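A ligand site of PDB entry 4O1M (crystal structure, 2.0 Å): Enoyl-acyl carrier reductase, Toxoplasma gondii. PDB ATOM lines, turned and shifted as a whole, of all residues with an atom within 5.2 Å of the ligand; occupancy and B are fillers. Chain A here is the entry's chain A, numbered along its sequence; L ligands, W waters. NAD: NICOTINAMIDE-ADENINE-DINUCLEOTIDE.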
ATOM      1  N   GLY A  16      23.909  -3.136  -7.618  1.00  0.00           N
ATOM      2  CA  GLY A  16      22.593  -3.288  -6.947  1.00  0.00           C
ATOM      3  C   GLY A  16      22.676  -4.198  -5.726  1.00  0.00           C
ATOM      4  O   GLY A  16      21.929  -5.194  -5.628  1.00  0.00           O
ATOM      5  N   VAL A  17      23.638  -3.927  -4.843  1.00  0.00           N
ATOM      6  CA  VAL A  17      23.787  -4.696  -3.625  1.00  0.00           C
ATOM      7  C   VAL A  17      23.820  -3.699  -2.485  1.00  0.00           C
ATOM      8  O   VAL A  17      24.768  -2.883  -2.383  1.00  0.00           O
ATOM      9  CB  VAL A  17      25.065  -5.532  -3.580  1.00  0.00           C
ATOM     10  CG1 VAL A  17      25.066  -6.418  -2.320  1.00  0.00           C
ATOM     11  CG2 VAL A  17      25.197  -6.434  -4.838  1.00  0.00           C
ATOM     12  N   ALA A  18      22.810  -3.783  -1.610  1.00  0.00           N
ATOM     13  CA  ALA A  18      22.706  -2.901  -0.447  1.00  0.00           C
ATOM     14  C   ALA A  18      22.497  -3.702   0.861  1.00  0.00           C
ATOM     15  O   ALA A  18      22.388  -3.122   1.935  1.00  0.00           O
ATOM     16  CB  ALA A  18      21.533  -1.905  -0.654  1.00  0.00           C
ATOM     17  N   ASP A  19      22.411  -5.030   0.760  1.00  0.00           N
ATOM     18  CA  ASP A  19      22.188  -5.851   1.958  1.00  0.00           C
ATOM     19  C   ASP A  19      22.361  -7.292   1.523  1.00  0.00           C
ATOM     20  O   ASP A  19      22.633  -7.543   0.352  1.00  0.00           O
ATOM     21  CB  ASP A  19      20.782  -5.649   2.511  1.00  0.00           C
ATOM     22  CG  ASP A  19      19.723  -5.846   1.439  1.00  0.00           C
ATOM     23  OD1 ASP A  19      19.513  -6.996   1.017  1.00  0.00           O
ATOM     24  OD2 ASP A  19      19.099  -4.847   1.015  1.00  0.00           O
ATOM     25  N   HIS A  21      20.105  -9.769   1.632  1.00  0.00           N
ATOM     26  CA  HIS A  21      18.833 -10.522   1.456  1.00  0.00           C
ATOM     27  C   HIS A  21      18.399 -10.704  -0.006  1.00  0.00           C
ATOM     28  O   HIS A  21      17.469 -11.457  -0.283  1.00  0.00           O
ATOM     29  CB  HIS A  21      17.702  -9.892   2.282  1.00  0.00           C
ATOM     30  CG  HIS A  21      17.952  -9.936   3.770  1.00  0.00           C
ATOM     31  ND1 HIS A  21      17.696 -11.038   4.551  1.00  0.00           N
ATOM     32  CD2 HIS A  21      18.471  -8.999   4.610  1.00  0.00           C
ATOM     33  CE1 HIS A  21      18.040 -10.792   5.806  1.00  0.00           C
ATOM     34  NE2 HIS A  21      18.494  -9.555   5.867  1.00  0.00           N
ATOM     35  N   GLY A  22      19.037  -9.988  -0.924  1.00  0.00           N
ATOM     36  CA  GLY A  22      18.574 -10.006  -2.311  1.00  0.00           C
ATOM     37  C   GLY A  22      19.368 -10.914  -3.227  1.00  0.00           C
ATOM     38  O   GLY A  22      20.323 -11.604  -2.797  1.00  0.00           O
ATOM     39  N   TYR A  23      18.964 -10.913  -4.498  1.00  0.00           N
ATOM     40  CA  TYR A  23      19.657 -11.740  -5.453  1.00  0.00           C
ATOM     41  C   TYR A  23      21.082 -11.254  -5.743  1.00  0.00           C
ATOM     42  O   TYR A  23      21.964 -12.061  -6.030  1.00  0.00           O
ATOM     43  CB  TYR A  23      18.853 -11.826  -6.755  1.00  0.00           C
ATOM     44  CG  TYR A  23      17.662 -12.773  -6.664  1.00  0.00           C
ATOM     45  CD1 TYR A  23      17.819 -14.098  -6.241  1.00  0.00           C
ATOM     46  CD2 TYR A  23      16.390 -12.351  -7.092  1.00  0.00           C
ATOM     47  CE1 TYR A  23      16.722 -14.959  -6.166  1.00  0.00           C
ATOM     48  CE2 TYR A  23      15.273 -13.230  -7.078  1.00  0.00           C
ATOM     49  CZ  TYR A  23      15.464 -14.536  -6.632  1.00  0.00           C
ATOM     50  OH  TYR A  23      14.406 -15.444  -6.629  1.00  0.00           O
ATOM     51  N   GLY A  24      21.279  -9.923  -5.669  1.00  0.00           N
ATOM     52  CA  GLY A  24      22.610  -9.311  -5.930  1.00  0.00           C
ATOM     53  C   GLY A  24      23.673  -9.897  -5.000  1.00  0.00           C
ATOM     54  O   GLY A  24      24.744 -10.303  -5.436  1.00  0.00           O
ATOM     55  N   THR A  42      26.453   0.301  -5.070  1.00  0.00           N
ATOM     56  CA  THR A  42      25.400   0.425  -4.064  1.00  0.00           C
ATOM     57  C   THR A  42      24.720   1.800  -4.210  1.00  0.00           C
ATOM     58  O   THR A  42      25.397   2.846  -4.279  1.00  0.00           O
ATOM     59  CB  THR A  42      26.035   0.306  -2.635  1.00  0.00           C
ATOM     60  OG1 THR A  42      26.697  -0.963  -2.469  1.00  0.00           O
ATOM     61  CG2 THR A  42      24.970   0.467  -1.564  1.00  0.00           C
ATOM     62  N   TRP A  43      23.396   1.804  -4.178  1.00  0.00           N
ATOM     63  CA  TRP A  43      22.618   3.060  -4.215  1.00  0.00           C
ATOM     64  C   TRP A  43      23.086   4.032  -3.102  1.00  0.00           C
ATOM     65  O   TRP A  43      23.111   3.653  -1.939  1.00  0.00           O
ATOM     66  CB  TRP A  43      21.113   2.697  -4.066  1.00  0.00           C
ATOM     67  CG  TRP A  43      20.198   3.838  -4.323  1.00  0.00           C
ATOM     68  CD1 TRP A  43      20.189   4.664  -5.428  1.00  0.00           C
ATOM     69  CD2 TRP A  43      19.118   4.284  -3.477  1.00  0.00           C
ATOM     70  NE1 TRP A  43      19.181   5.603  -5.297  1.00  0.00           N
ATOM     71  CE2 TRP A  43      18.513   5.396  -4.109  1.00  0.00           C
ATOM     72  CE3 TRP A  43      18.614   3.860  -2.232  1.00  0.00           C
ATOM     73  CZ2 TRP A  43      17.424   6.100  -3.546  1.00  0.00           C
ATOM     74  CZ3 TRP A  43      17.533   4.569  -1.659  1.00  0.00           C
ATOM     75  CH2 TRP A  43      16.950   5.665  -2.327  1.00  0.00           C
ATOM     76  N   VAL A  46      21.895   4.418   0.715  1.00  0.00           N
ATOM     77  CA  VAL A  46      22.042   3.302   1.666  1.00  0.00           C
ATOM     78  C   VAL A  46      23.468   2.753   1.768  1.00  0.00           C
ATOM     79  O   VAL A  46      23.690   1.704   2.370  1.00  0.00           O
ATOM     80  CB  VAL A  46      21.036   2.147   1.381  1.00  0.00           C
ATOM     81  CG1 VAL A  46      19.600   2.626   1.536  1.00  0.00           C
ATOM     82  CG2 VAL A  46      21.282   1.522  -0.016  1.00  0.00           C
ATOM     83  N   LEU A  79      26.700   4.108  -6.411  1.00  0.00           N
ATOM     84  CA  LEU A  79      26.214   4.045  -7.798  1.00  0.00           C
ATOM     85  C   LEU A  79      24.717   4.336  -7.848  1.00  0.00           C
ATOM     86  O   LEU A  79      23.902   3.629  -7.246  1.00  0.00           O
ATOM     87  CB  LEU A  79      26.501   2.677  -8.417  1.00  0.00           C
ATOM     88  CG  LEU A  79      25.833   2.336  -9.764  1.00  0.00           C
ATOM     89  CD1 LEU A  79      26.273   3.269 -10.873  1.00  0.00           C
ATOM     90  CD2 LEU A  79      26.094   0.887 -10.147  1.00  0.00           C
ATOM     91  N   ASP A  80      24.355   5.395  -8.558  1.00  0.00           N
ATOM     92  CA  ASP A  80      22.948   5.647  -8.797  1.00  0.00           C
ATOM     93  C   ASP A  80      22.658   5.442 -10.271  1.00  0.00           C
ATOM     94  O   ASP A  80      22.980   6.276 -11.124  1.00  0.00           O
ATOM     95  CB  ASP A  80      22.497   7.050  -8.272  1.00  0.00           C
ATOM     96  CG  ASP A  80      20.963   7.198  -8.265  1.00  0.00           C
ATOM     97  OD1 ASP A  80      20.294   6.608  -9.139  1.00  0.00           O
ATOM     98  OD2 ASP A  80      20.436   7.930  -7.425  1.00  0.00           O
ATOM     99  N   ALA A  81      22.038   4.296 -10.571  1.00  0.00           N
ATOM    100  CA  ALA A  81      21.786   3.899 -11.945  1.00  0.00           C
ATOM    101  C   ALA A  81      20.729   4.722 -12.690  1.00  0.00           C
ATOM    102  O   ALA A  81      20.491   4.448 -13.859  1.00  0.00           O
ATOM    103  CB  ALA A  81      21.437   2.391 -11.993  1.00  0.00           C
ATOM    104  N   ALA A  82      20.122   5.727 -12.032  1.00  0.00           N
ATOM    105  CA  ALA A  82      19.212   6.688 -12.669  1.00  0.00           C
ATOM    106  C   ALA A  82      19.991   7.740 -13.463  1.00  0.00           C
ATOM    107  O   ALA A  82      19.393   8.446 -14.266  1.00  0.00           O
ATOM    108  CB  ALA A  82      18.317   7.388 -11.628  1.00  0.00           C
ATOM    109  N   SER A 127      21.633  -6.154 -10.964  1.00  0.00           N
ATOM    110  CA  SER A 127      20.639  -6.725 -10.050  1.00  0.00           C
ATOM    111  C   SER A 127      19.909  -5.584  -9.356  1.00  0.00           C
ATOM    112  O   SER A 127      19.989  -5.431  -8.136  1.00  0.00           O
ATOM    113  CB  SER A 127      21.334  -7.570  -8.963  1.00  0.00           C
ATOM    114  OG  SER A 127      20.336  -8.187  -8.137  1.00  0.00           O
ATOM    115  N   LEU A 128      19.229  -4.757 -10.127  1.00  0.00           N
ATOM    116  CA  LEU A 128      18.626  -3.553  -9.574  1.00  0.00           C
ATOM    117  C   LEU A 128      17.363  -3.190 -10.310  1.00  0.00           C
ATOM    118  O   LEU A 128      17.242  -3.447 -11.506  1.00  0.00           O
ATOM    119  CB  LEU A 128      19.606  -2.390  -9.556  1.00  0.00           C
ATOM    120  CG  LEU A 128      20.098  -1.723 -10.840  1.00  0.00           C
ATOM    121  CD1 LEU A 128      19.157  -0.616 -11.270  1.00  0.00           C
ATOM    122  CD2 LEU A 128      21.493  -1.133 -10.566  1.00  0.00           C
ATOM    123  N   ALA A 129      16.398  -2.662  -9.577  1.00  0.00           N
ATOM    124  CA  ALA A 129      15.105  -2.305 -10.174  1.00  0.00           C
ATOM    125  C   ALA A 129      14.452  -1.349  -9.224  1.00  0.00           C
ATOM    126  O   ALA A 129      14.751  -1.398  -8.023  1.00  0.00           O
ATOM    127  CB  ALA A 129      14.229  -3.549 -10.325  1.00  0.00           C
ATOM    128  N   ASN A 130      13.588  -0.507  -9.735  1.00  0.00           N
ATOM    129  CA  ASN A 130      12.835   0.376  -8.903  1.00  0.00           C
ATOM    130  C   ASN A 130      11.636   0.896  -9.693  1.00  0.00           C
ATOM    131  O   ASN A 130      11.795   1.526 -10.762  1.00  0.00           O
ATOM    132  CB  ASN A 130      13.701   1.530  -8.392  1.00  0.00           C
ATOM    133  CG  ASN A 130      12.916   2.523  -7.532  1.00  0.00           C
ATOM    134  OD1 ASN A 130      13.016   3.731  -7.723  1.00  0.00           O
ATOM    135  ND2 ASN A 130      12.152   2.020  -6.575  1.00  0.00           N
ATOM    136  N   ASN A 152      14.904   3.353 -14.336  1.00  0.00           N
ATOM    137  CA  ASN A 152      15.621   2.696 -13.240  1.00  0.00           C
ATOM    138  C   ASN A 152      15.947   1.205 -13.501  1.00  0.00           C
ATOM    139  O   ASN A 152      16.980   0.727 -13.078  1.00  0.00           O
ATOM    140  CB  ASN A 152      14.781   2.744 -11.961  1.00  0.00           C
ATOM    141  CG  ASN A 152      14.563   4.151 -11.458  1.00  0.00           C
ATOM    142  OD1 ASN A 152      15.391   5.017 -11.657  1.00  0.00           O
ATOM    143  ND2 ASN A 152      13.410   4.384 -10.796  1.00  0.00           N
ATOM    144  N   LEU A 177      18.465  -9.506 -14.221  1.00  0.00           N
ATOM    145  CA  LEU A 177      17.393 -10.290 -13.562  1.00  0.00           C
ATOM    146  C   LEU A 177      16.046  -9.780 -13.985  1.00  0.00           C
ATOM    147  O   LEU A 177      15.777  -8.580 -13.958  1.00  0.00           O
ATOM    148  CB  LEU A 177      17.525 -10.229 -12.046  1.00  0.00           C
ATOM    149  CG  LEU A 177      18.769 -10.962 -11.518  1.00  0.00           C
ATOM    150  CD1 LEU A 177      19.094 -10.606 -10.122  1.00  0.00           C
ATOM    151  CD2 LEU A 177      18.535 -12.453 -11.584  1.00  0.00           C
ATOM    152  N   SER A 178      15.186 -10.712 -14.351  1.00  0.00           N
ATOM    153  CA  SER A 178      13.874 -10.382 -14.837  1.00  0.00           C
ATOM    154  C   SER A 178      12.842 -11.268 -14.085  1.00  0.00           C
ATOM    155  O   SER A 178      13.173 -11.993 -13.162  1.00  0.00           O
ATOM    156  CB  SER A 178      13.796 -10.652 -16.361  1.00  0.00           C
ATOM    157  OG  SER A 178      12.553 -10.159 -16.861  1.00  0.00           O
ATOM    158  N   TYR A 179      11.591 -11.216 -14.532  1.00  0.00           N
ATOM    159  CA  TYR A 179      10.521 -11.932 -13.869  1.00  0.00           C
ATOM    160  C   TYR A 179       9.475 -12.276 -14.928  1.00  0.00           C
ATOM    161  O   TYR A 179       9.338 -11.527 -15.921  1.00  0.00           O
ATOM    162  CB  TYR A 179       9.946 -11.083 -12.730  1.00  0.00           C
ATOM    163  CG  TYR A 179       8.794 -11.736 -11.980  1.00  0.00           C
ATOM    164  CD1 TYR A 179       8.942 -13.000 -11.401  1.00  0.00           C
ATOM    165  CD2 TYR A 179       7.589 -11.087 -11.841  1.00  0.00           C
ATOM    166  CE1 TYR A 179       7.900 -13.636 -10.731  1.00  0.00           C
ATOM    167  CE2 TYR A 179       6.509 -11.670 -11.149  1.00  0.00           C
ATOM    168  CZ  TYR A 179       6.668 -12.948 -10.628  1.00  0.00           C
ATOM    169  OH  TYR A 179       5.626 -13.493  -9.944  1.00  0.00           O
ATOM    170  N   TYR A 189       2.067  -7.132  -9.897  1.00  0.00           N
ATOM    171  CA  TYR A 189       3.371  -6.599 -10.327  1.00  0.00           C
ATOM    172  C   TYR A 189       3.096  -5.398 -11.279  1.00  0.00           C
ATOM    173  O   TYR A 189       3.093  -5.527 -12.502  1.00  0.00           O
ATOM    174  CB  TYR A 189       4.191  -7.697 -11.013  1.00  0.00           C
ATOM    175  CG  TYR A 189       5.650  -7.362 -11.126  1.00  0.00           C
ATOM    176  CD1 TYR A 189       6.432  -7.152  -9.997  1.00  0.00           C
ATOM    177  CD2 TYR A 189       6.247  -7.229 -12.377  1.00  0.00           C
ATOM    178  CE1 TYR A 189       7.811  -6.856 -10.127  1.00  0.00           C
ATOM    179  CE2 TYR A 189       7.606  -6.956 -12.528  1.00  0.00           C
ATOM    180  CZ  TYR A 189       8.366  -6.746 -11.402  1.00  0.00           C
ATOM    181  OH  TYR A 189       9.706  -6.481 -11.554  1.00  0.00           O
ATOM    182  N   MET A 193       6.177  -2.107 -14.160  1.00  0.00           N
ATOM    183  CA  MET A 193       7.346  -2.935 -13.926  1.00  0.00           C
ATOM    184  C   MET A 193       7.303  -4.162 -14.838  1.00  0.00           C
ATOM    185  O   MET A 193       8.354  -4.650 -15.240  1.00  0.00           O
ATOM    186  CB  MET A 193       7.473  -3.371 -12.464  1.00  0.00           C
ATOM    187  CG  MET A 193       7.986  -2.317 -11.553  1.00  0.00           C
ATOM    188  SD  MET A 193       9.613  -1.699 -11.960  1.00  0.00           S
ATOM    189  CE  MET A 193      10.645  -3.177 -11.976  1.00  0.00           C
ATOM    190  N   LYS A 197      10.372  -4.993 -17.406  1.00  0.00           N
ATOM    191  CA  LYS A 197      11.059  -6.265 -17.509  1.00  0.00           C
ATOM    192  C   LYS A 197      10.984  -6.841 -18.929  1.00  0.00           C
ATOM    193  O   LYS A 197      11.936  -7.460 -19.383  1.00  0.00           O
ATOM    194  CB  LYS A 197      10.502  -7.286 -16.498  1.00  0.00           C
ATOM    195  CG  LYS A 197      10.776  -6.910 -15.019  1.00  0.00           C
ATOM    196  CD  LYS A 197      12.283  -6.625 -14.759  1.00  0.00           C
ATOM    197  CE  LYS A 197      12.618  -6.691 -13.229  1.00  0.00           C
ATOM    198  NZ  LYS A 197      14.098  -6.643 -12.903  1.00  0.00           N
ATOM    199  N   ALA A 224      13.779 -14.915 -12.553  1.00  0.00           N
ATOM    200  CA  ALA A 224      13.787 -15.539 -11.252  1.00  0.00           C
ATOM    201  C   ALA A 224      12.375 -15.659 -10.675  1.00  0.00           C
ATOM    202  O   ALA A 224      11.447 -14.939 -11.054  1.00  0.00           O
ATOM    203  CB  ALA A 224      14.674 -14.741 -10.317  1.00  0.00           C
ATOM    204  N   GLY A 225      12.211 -16.601  -9.764  1.00  0.00           N
ATOM    205  CA  GLY A 225      10.976 -16.688  -8.967  1.00  0.00           C
ATOM    206  C   GLY A 225      10.960 -15.740  -7.768  1.00  0.00           C
ATOM    207  O   GLY A 225      11.928 -15.016  -7.515  1.00  0.00           O
ATOM    208  N   PRO A 226       9.862 -15.757  -7.010  1.00  0.00           N
ATOM    209  CA  PRO A 226       9.701 -14.789  -5.911  1.00  0.00           C
ATOM    210  C   PRO A 226      10.629 -15.084  -4.747  1.00  0.00           C
ATOM    211  O   PRO A 226      10.837 -16.271  -4.379  1.00  0.00           O
ATOM    212  CB  PRO A 226       8.223 -14.956  -5.460  1.00  0.00           C
ATOM    213  CG  PRO A 226       7.640 -16.036  -6.316  1.00  0.00           C
ATOM    214  CD  PRO A 226       8.667 -16.592  -7.231  1.00  0.00           C
ATOM    215  N   LEU A 227      11.184 -14.011  -4.176  1.00  0.00           N
ATOM    216  CA  LEU A 227      12.172 -14.066  -3.084  1.00  0.00           C
ATOM    217  C   LEU A 227      11.823 -12.965  -2.089  1.00  0.00           C
ATOM    218  O   LEU A 227      11.524 -11.813  -2.485  1.00  0.00           O
ATOM    219  CB  LEU A 227      13.588 -13.826  -3.609  1.00  0.00           C
ATOM    220  CG  LEU A 227      14.699 -13.739  -2.533  1.00  0.00           C
ATOM    221  CD1 LEU A 227      15.063 -15.161  -2.057  1.00  0.00           C
ATOM    222  CD2 LEU A 227      15.920 -13.030  -3.106  1.00  0.00           C
ATOM    223  N   LYS A 228      11.884 -13.300  -0.803  1.00  0.00           N
ATOM    224  CA  LYS A 228      11.582 -12.304   0.236  1.00  0.00           C
ATOM    225  C   LYS A 228      12.817 -11.399   0.517  1.00  0.00           C
ATOM    226  O   LYS A 228      13.435 -11.441   1.575  1.00  0.00           O
ATOM    227  CB  LYS A 228      11.003 -12.970   1.500  1.00  0.00           C
ATOM    228  CG  LYS A 228      10.197 -12.006   2.380  1.00  0.00           C
ATOM    229  CD  LYS A 228       9.691 -12.685   3.624  1.00  0.00           C
ATOM    230  CE  LYS A 228       9.048 -11.680   4.581  1.00  0.00           C
ATOM    231  NZ  LYS A 228       7.578 -11.555   4.354  1.00  0.00           N
ATOM    232  N   SER A 229      13.174 -10.590  -0.481  1.00  0.00           N
ATOM    233  CA  SER A 229      14.244  -9.637  -0.355  1.00  0.00           C
ATOM    234  C   SER A 229      13.745  -8.448   0.485  1.00  0.00           C
ATOM    235  O   SER A 229      12.553  -8.354   0.819  1.00  0.00           O
ATOM    236  CB  SER A 229      14.663  -9.195  -1.752  1.00  0.00           C
ATOM    237  OG  SER A 229      13.572  -8.530  -2.398  1.00  0.00           O
ATOM    238  N   ARG A 230      14.642  -7.515   0.804  1.00  0.00           N
ATOM    239  CA  ARG A 230      14.179  -6.299   1.474  1.00  0.00           C
ATOM    240  C   ARG A 230      13.261  -5.457   0.552  1.00  0.00           C
ATOM    241  O   ARG A 230      12.213  -4.961   0.994  1.00  0.00           O
ATOM    242  CB  ARG A 230      15.345  -5.481   2.006  1.00  0.00           C
ATOM    243  CG  ARG A 230      15.940  -6.073   3.264  1.00  0.00           C
ATOM    244  CD  ARG A 230      16.281  -5.005   4.284  1.00  0.00           C
ATOM    245  NE  ARG A 230      16.723  -5.624   5.536  1.00  0.00           N
ATOM    246  CZ  ARG A 230      17.968  -5.575   6.015  1.00  0.00           C
ATOM    247  NH1 ARG A 230      18.922  -4.898   5.381  1.00  0.00           N
ATOM    248  NH2 ARG A 230      18.260  -6.187   7.168  1.00  0.00           N
ATOM    249  N   ALA A 231      13.643  -5.292  -0.708  1.00  0.00           N
ATOM    250  CA  ALA A 231      12.767  -4.579  -1.665  1.00  0.00           C
ATOM    251  C   ALA A 231      11.358  -5.203  -1.726  1.00  0.00           C
ATOM    252  O   ALA A 231      10.327  -4.478  -1.703  1.00  0.00           O
ATOM    253  CB  ALA A 231      13.398  -4.540  -3.067  1.00  0.00           C
ATOM    254  N   ALA A 232      11.289  -6.551  -1.783  1.00  0.00           N
ATOM    255  CA  ALA A 232      10.009  -7.252  -1.873  1.00  0.00           C
ATOM    256  C   ALA A 232       9.148  -7.159  -0.600  1.00  0.00           C
ATOM    257  O   ALA A 232       7.946  -6.948  -0.680  1.00  0.00           O
ATOM    258  CB  ALA A 232      10.228  -8.747  -2.289  1.00  0.00           C
ATOM    259  N   ILE A 244       4.357 -10.514  -0.890  1.00  0.00           N
ATOM    260  CA  ILE A 244       5.447 -11.364  -1.310  1.00  0.00           C
ATOM    261  C   ILE A 244       5.221 -12.770  -0.755  1.00  0.00           C
ATOM    262  O   ILE A 244       5.573 -13.726  -1.418  1.00  0.00           O
ATOM    263  CB  ILE A 244       6.865 -10.823  -0.898  1.00  0.00           C
ATOM    264  CG1 ILE A 244       7.966 -11.771  -1.421  1.00  0.00           C
ATOM    265  CG2 ILE A 244       7.008 -10.675   0.653  1.00  0.00           C
ATOM    266  CD1 ILE A 244       7.919 -11.990  -2.925  1.00  0.00           C
HETATM  267  PA  NAD L   1      16.914  -5.833  -3.465  1.00  0.00           P
HETATM  268  O1A NAD L   1      16.286  -5.966  -2.106  1.00  0.00           O
HETATM  269  O2A NAD L   1      18.358  -6.099  -3.716  1.00  0.00           O
HETATM  270  O5B NAD L   1      16.512  -4.363  -4.030  1.00  0.00           O
HETATM  271  C5B NAD L   1      16.812  -3.982  -5.386  1.00  0.00           C
HETATM  272  C4B NAD L   1      18.222  -3.392  -5.413  1.00  0.00           C
HETATM  273  O4B NAD L   1      18.257  -2.352  -6.397  1.00  0.00           O
HETATM  274  C3B NAD L   1      18.681  -2.719  -4.096  1.00  0.00           C
HETATM  275  O3B NAD L   1      20.073  -3.072  -3.902  1.00  0.00           O
HETATM  276  C2B NAD L   1      18.574  -1.236  -4.424  1.00  0.00           C
HETATM  277  O2B NAD L   1      19.449  -0.386  -3.637  1.00  0.00           O
HETATM  278  C1B NAD L   1      19.021  -1.289  -5.882  1.00  0.00           C
HETATM  279  N9A NAD L   1      18.612  -0.061  -6.580  1.00  0.00           N
HETATM  280  C8A NAD L   1      17.341   0.384  -6.756  1.00  0.00           C
HETATM  281  N7A NAD L   1      17.404   1.568  -7.415  1.00  0.00           N
HETATM  282  C5A NAD L   1      18.730   1.828  -7.639  1.00  0.00           C
HETATM  283  C6A NAD L   1      19.480   2.918  -8.299  1.00  0.00           C
HETATM  284  N6A NAD L   1      18.842   3.993  -8.851  1.00  0.00           N
HETATM  285  N1A NAD L   1      20.835   2.843  -8.302  1.00  0.00           N
HETATM  286  C2A NAD L   1      21.514   1.805  -7.778  1.00  0.00           C
HETATM  287  N3A NAD L   1      20.852   0.794  -7.164  1.00  0.00           N
HETATM  288  C4A NAD L   1      19.483   0.793  -7.096  1.00  0.00           C
HETATM  289  O3  NAD L   1      16.039  -6.551  -4.596  1.00  0.00           O
HETATM  290  PN  NAD L   1      15.860  -8.054  -5.109  1.00  0.00           P
HETATM  291  O1N NAD L   1      14.386  -8.338  -4.972  1.00  0.00           O
HETATM  292  O2N NAD L   1      16.906  -9.037  -4.777  1.00  0.00           O
HETATM  293  O5D NAD L   1      15.974  -7.687  -6.679  1.00  0.00           O
HETATM  294  C5D NAD L   1      17.154  -7.693  -7.486  1.00  0.00           C
HETATM  295  C4D NAD L   1      16.698  -7.950  -8.936  1.00  0.00           C
HETATM  296  O4D NAD L   1      15.990  -9.198  -8.946  1.00  0.00           O
HETATM  297  C3D NAD L   1      15.686  -6.910  -9.450  1.00  0.00           C
HETATM  298  O3D NAD L   1      15.963  -6.619 -10.822  1.00  0.00           O
HETATM  299  C2D NAD L   1      14.336  -7.572  -9.339  1.00  0.00           C
HETATM  300  O2D NAD L   1      13.329  -7.082 -10.265  1.00  0.00           O
HETATM  301  C1D NAD L   1      14.711  -9.051  -9.585  1.00  0.00           C
HETATM  302  N1N NAD L   1      13.695  -9.989  -9.121  1.00  0.00           N
HETATM  303  C2N NAD L   1      13.279  -9.998  -7.816  1.00  0.00           C
HETATM  304  C3N NAD L   1      12.269 -10.844  -7.419  1.00  0.00           C
HETATM  305  C7N NAD L   1      11.833 -10.953  -5.968  1.00  0.00           C
HETATM  306  O7N NAD L   1      12.496 -10.458  -5.027  1.00  0.00           O
HETATM  307  N7N NAD L   1      10.788 -11.716  -5.742  1.00  0.00           N
HETATM  308  C4N NAD L   1      11.661 -11.691  -8.356  1.00  0.00           C
HETATM  309  C5N NAD L   1      12.144 -11.706  -9.661  1.00  0.00           C
HETATM  310  C6N NAD L   1      13.143 -10.819 -10.033  1.00  0.00           C
HETATM  311  O   HOH W   1      18.075  -6.540 -12.645  1.00  0.00           O
HETATM  312  O   HOH W   2      21.984  -0.607  -4.325  1.00  0.00           O
HETATM  313  O   HOH W   3      11.211  -5.854  -9.361  1.00  0.00           O
HETATM  314  O   HOH W   4      12.353  -6.864  -5.945  1.00  0.00           O
HETATM  315  O   HOH W   5      17.283  -7.389  -0.312  1.00  0.00           O
HETATM  316  O   HOH W   6      20.066  -7.294  -5.460  1.00  0.00           O
HETATM  317  O   HOH W   7      20.396  -5.402  -1.928  1.00  0.00           O
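The side-chain hydroxyl (OG) of Ser 127 is in hydrogen-bond range of the backbone NH (N) of Gly 24, 3.2 Å away.
The side-chain amide oxygen of Asn 130 sits at hydrogen-bond distance from the side-chain amide nitrogen of Asn 152.
The backbone NH (N) of Ala 232 sits at hydrogen-bond distance from the side-chain hydroxyl (OG) of Ser 229, at 3.1 Å.
The backbone carbonyl oxygen (O) of Val 17 sits at hydrogen-bond distance from the side-chain hydroxyl (OG1) of Thr 42 (2.7 Å).
OH of Tyr 23 sits at hydrogen-bond distance from O of Gly 225, 2.7 Å away.
The side-chain amino group (NZ) of Lys 197 is in hydrogen-bond range of the backbone carbonyl oxygen (O) of Leu 177 (2.8 Å).
O of Thr 42 is in hydrogen-bond range of N of Leu 79 (2.8 Å).
OD2 of Asp 80 sits at hydrogen-bond distance from NE1 of Trp 43, at 3.4 Å.
N7N of the ligand sits at hydrogen-bond distance from O of Leu 227 (3.3 Å).
The backbone NH of Tyr 23 sits at hydrogen-bond distance from an oxygen (O2N) of the ligand, 2.8 Å away.
N of Ala 231 lies within hydrogen-bond range of O1A of the ligand (3.1 Å).
O of Leu 128 lies within hydrogen-bond range of O3D of the ligand, at 3.5 Å.
N1A of the ligand sits at hydrogen-bond distance from N of Ala 81, 3.0 Å away.
O3B of the ligand sits at hydrogen-bond distance from O of Gly 16 (3.3 Å).
The side-chain carboxylate (OD1) of Asp 80 sits at hydrogen-bond distance from a nitrogen (N6A) of the ligand (3.0 Å).
An oxygen (O2D) of the ligand lies within hydrogen-bond range of the side-chain amino group (NZ) of Lys 197, 2.8 Å away.
The side-chain hydroxyl of Ser 229 lies within hydrogen-bond range of an oxygen (O1N) of the ligand (2.7 Å).
A nitrogen (N1A) of the ligand lies close to the backbone carbonyl oxygen of Leu 79 (3.3 Å).
Merely in contact with the ligand: Val 17, Ala 18, Gly 22, Trp 43, Ala 82, Ser 127, Ala 129, Asn 130, Leu 177, Ser 178, Tyr 179, Tyr 189, Ala 224, Gly 225, Pro 226, Arg 230 and Ala 232.
Hydrophobic or aromatic side chains within 4 Å of the ligand: Ala 18, Tyr 23, Trp 43, Ala 81, Leu 128, Ala 129, Leu 177, Tyr 179, Leu 227, Ala 231 and Ala 232.
Of the 36 residues printed, 27 come within 4 Å of the ligand.
Water W5 lies within hydrogen-bond range of an oxygen (O1A) of the ligand (2.5 Å), the side-chain carboxylate (OD1) of Asp 19 (2.6 Å), the backbone NH (N) of Arg 230 (2.9 Å) and the backbone NH (N) of Gly 22 (3.2 Å).
Water W3 lies within hydrogen-bond range of O2D of the ligand (2.6 Å) and OH of Tyr 189 (2.7 Å).
Water W2 lies within hydrogen-bond range of O2B of the ligand (2.6 Å) and N of Trp 43 (2.8 Å).
Water W6 lies within hydrogen-bond range of O2A of the ligand (2.7 Å), O of Gly 16 (2.8 Å), OG of Ser 127 (2.8 Å) and N of Gly 24 (2.9 Å).
Water W1 lies within hydrogen-bond range of an oxygen (O3D) of the ligand (2.8 Å), the backbone NH (N) of Leu 128 (3.3 Å) and the backbone carbonyl oxygen (O) of Leu 177 (3.3 Å).
Water W7 lies within hydrogen-bond range of an oxygen (O2A) of the ligand (2.8 Å), the backbone NH (N) of Ala 18 (2.9 Å) and the side-chain carboxylate (OD2) of Asp 19 (3.3 Å).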
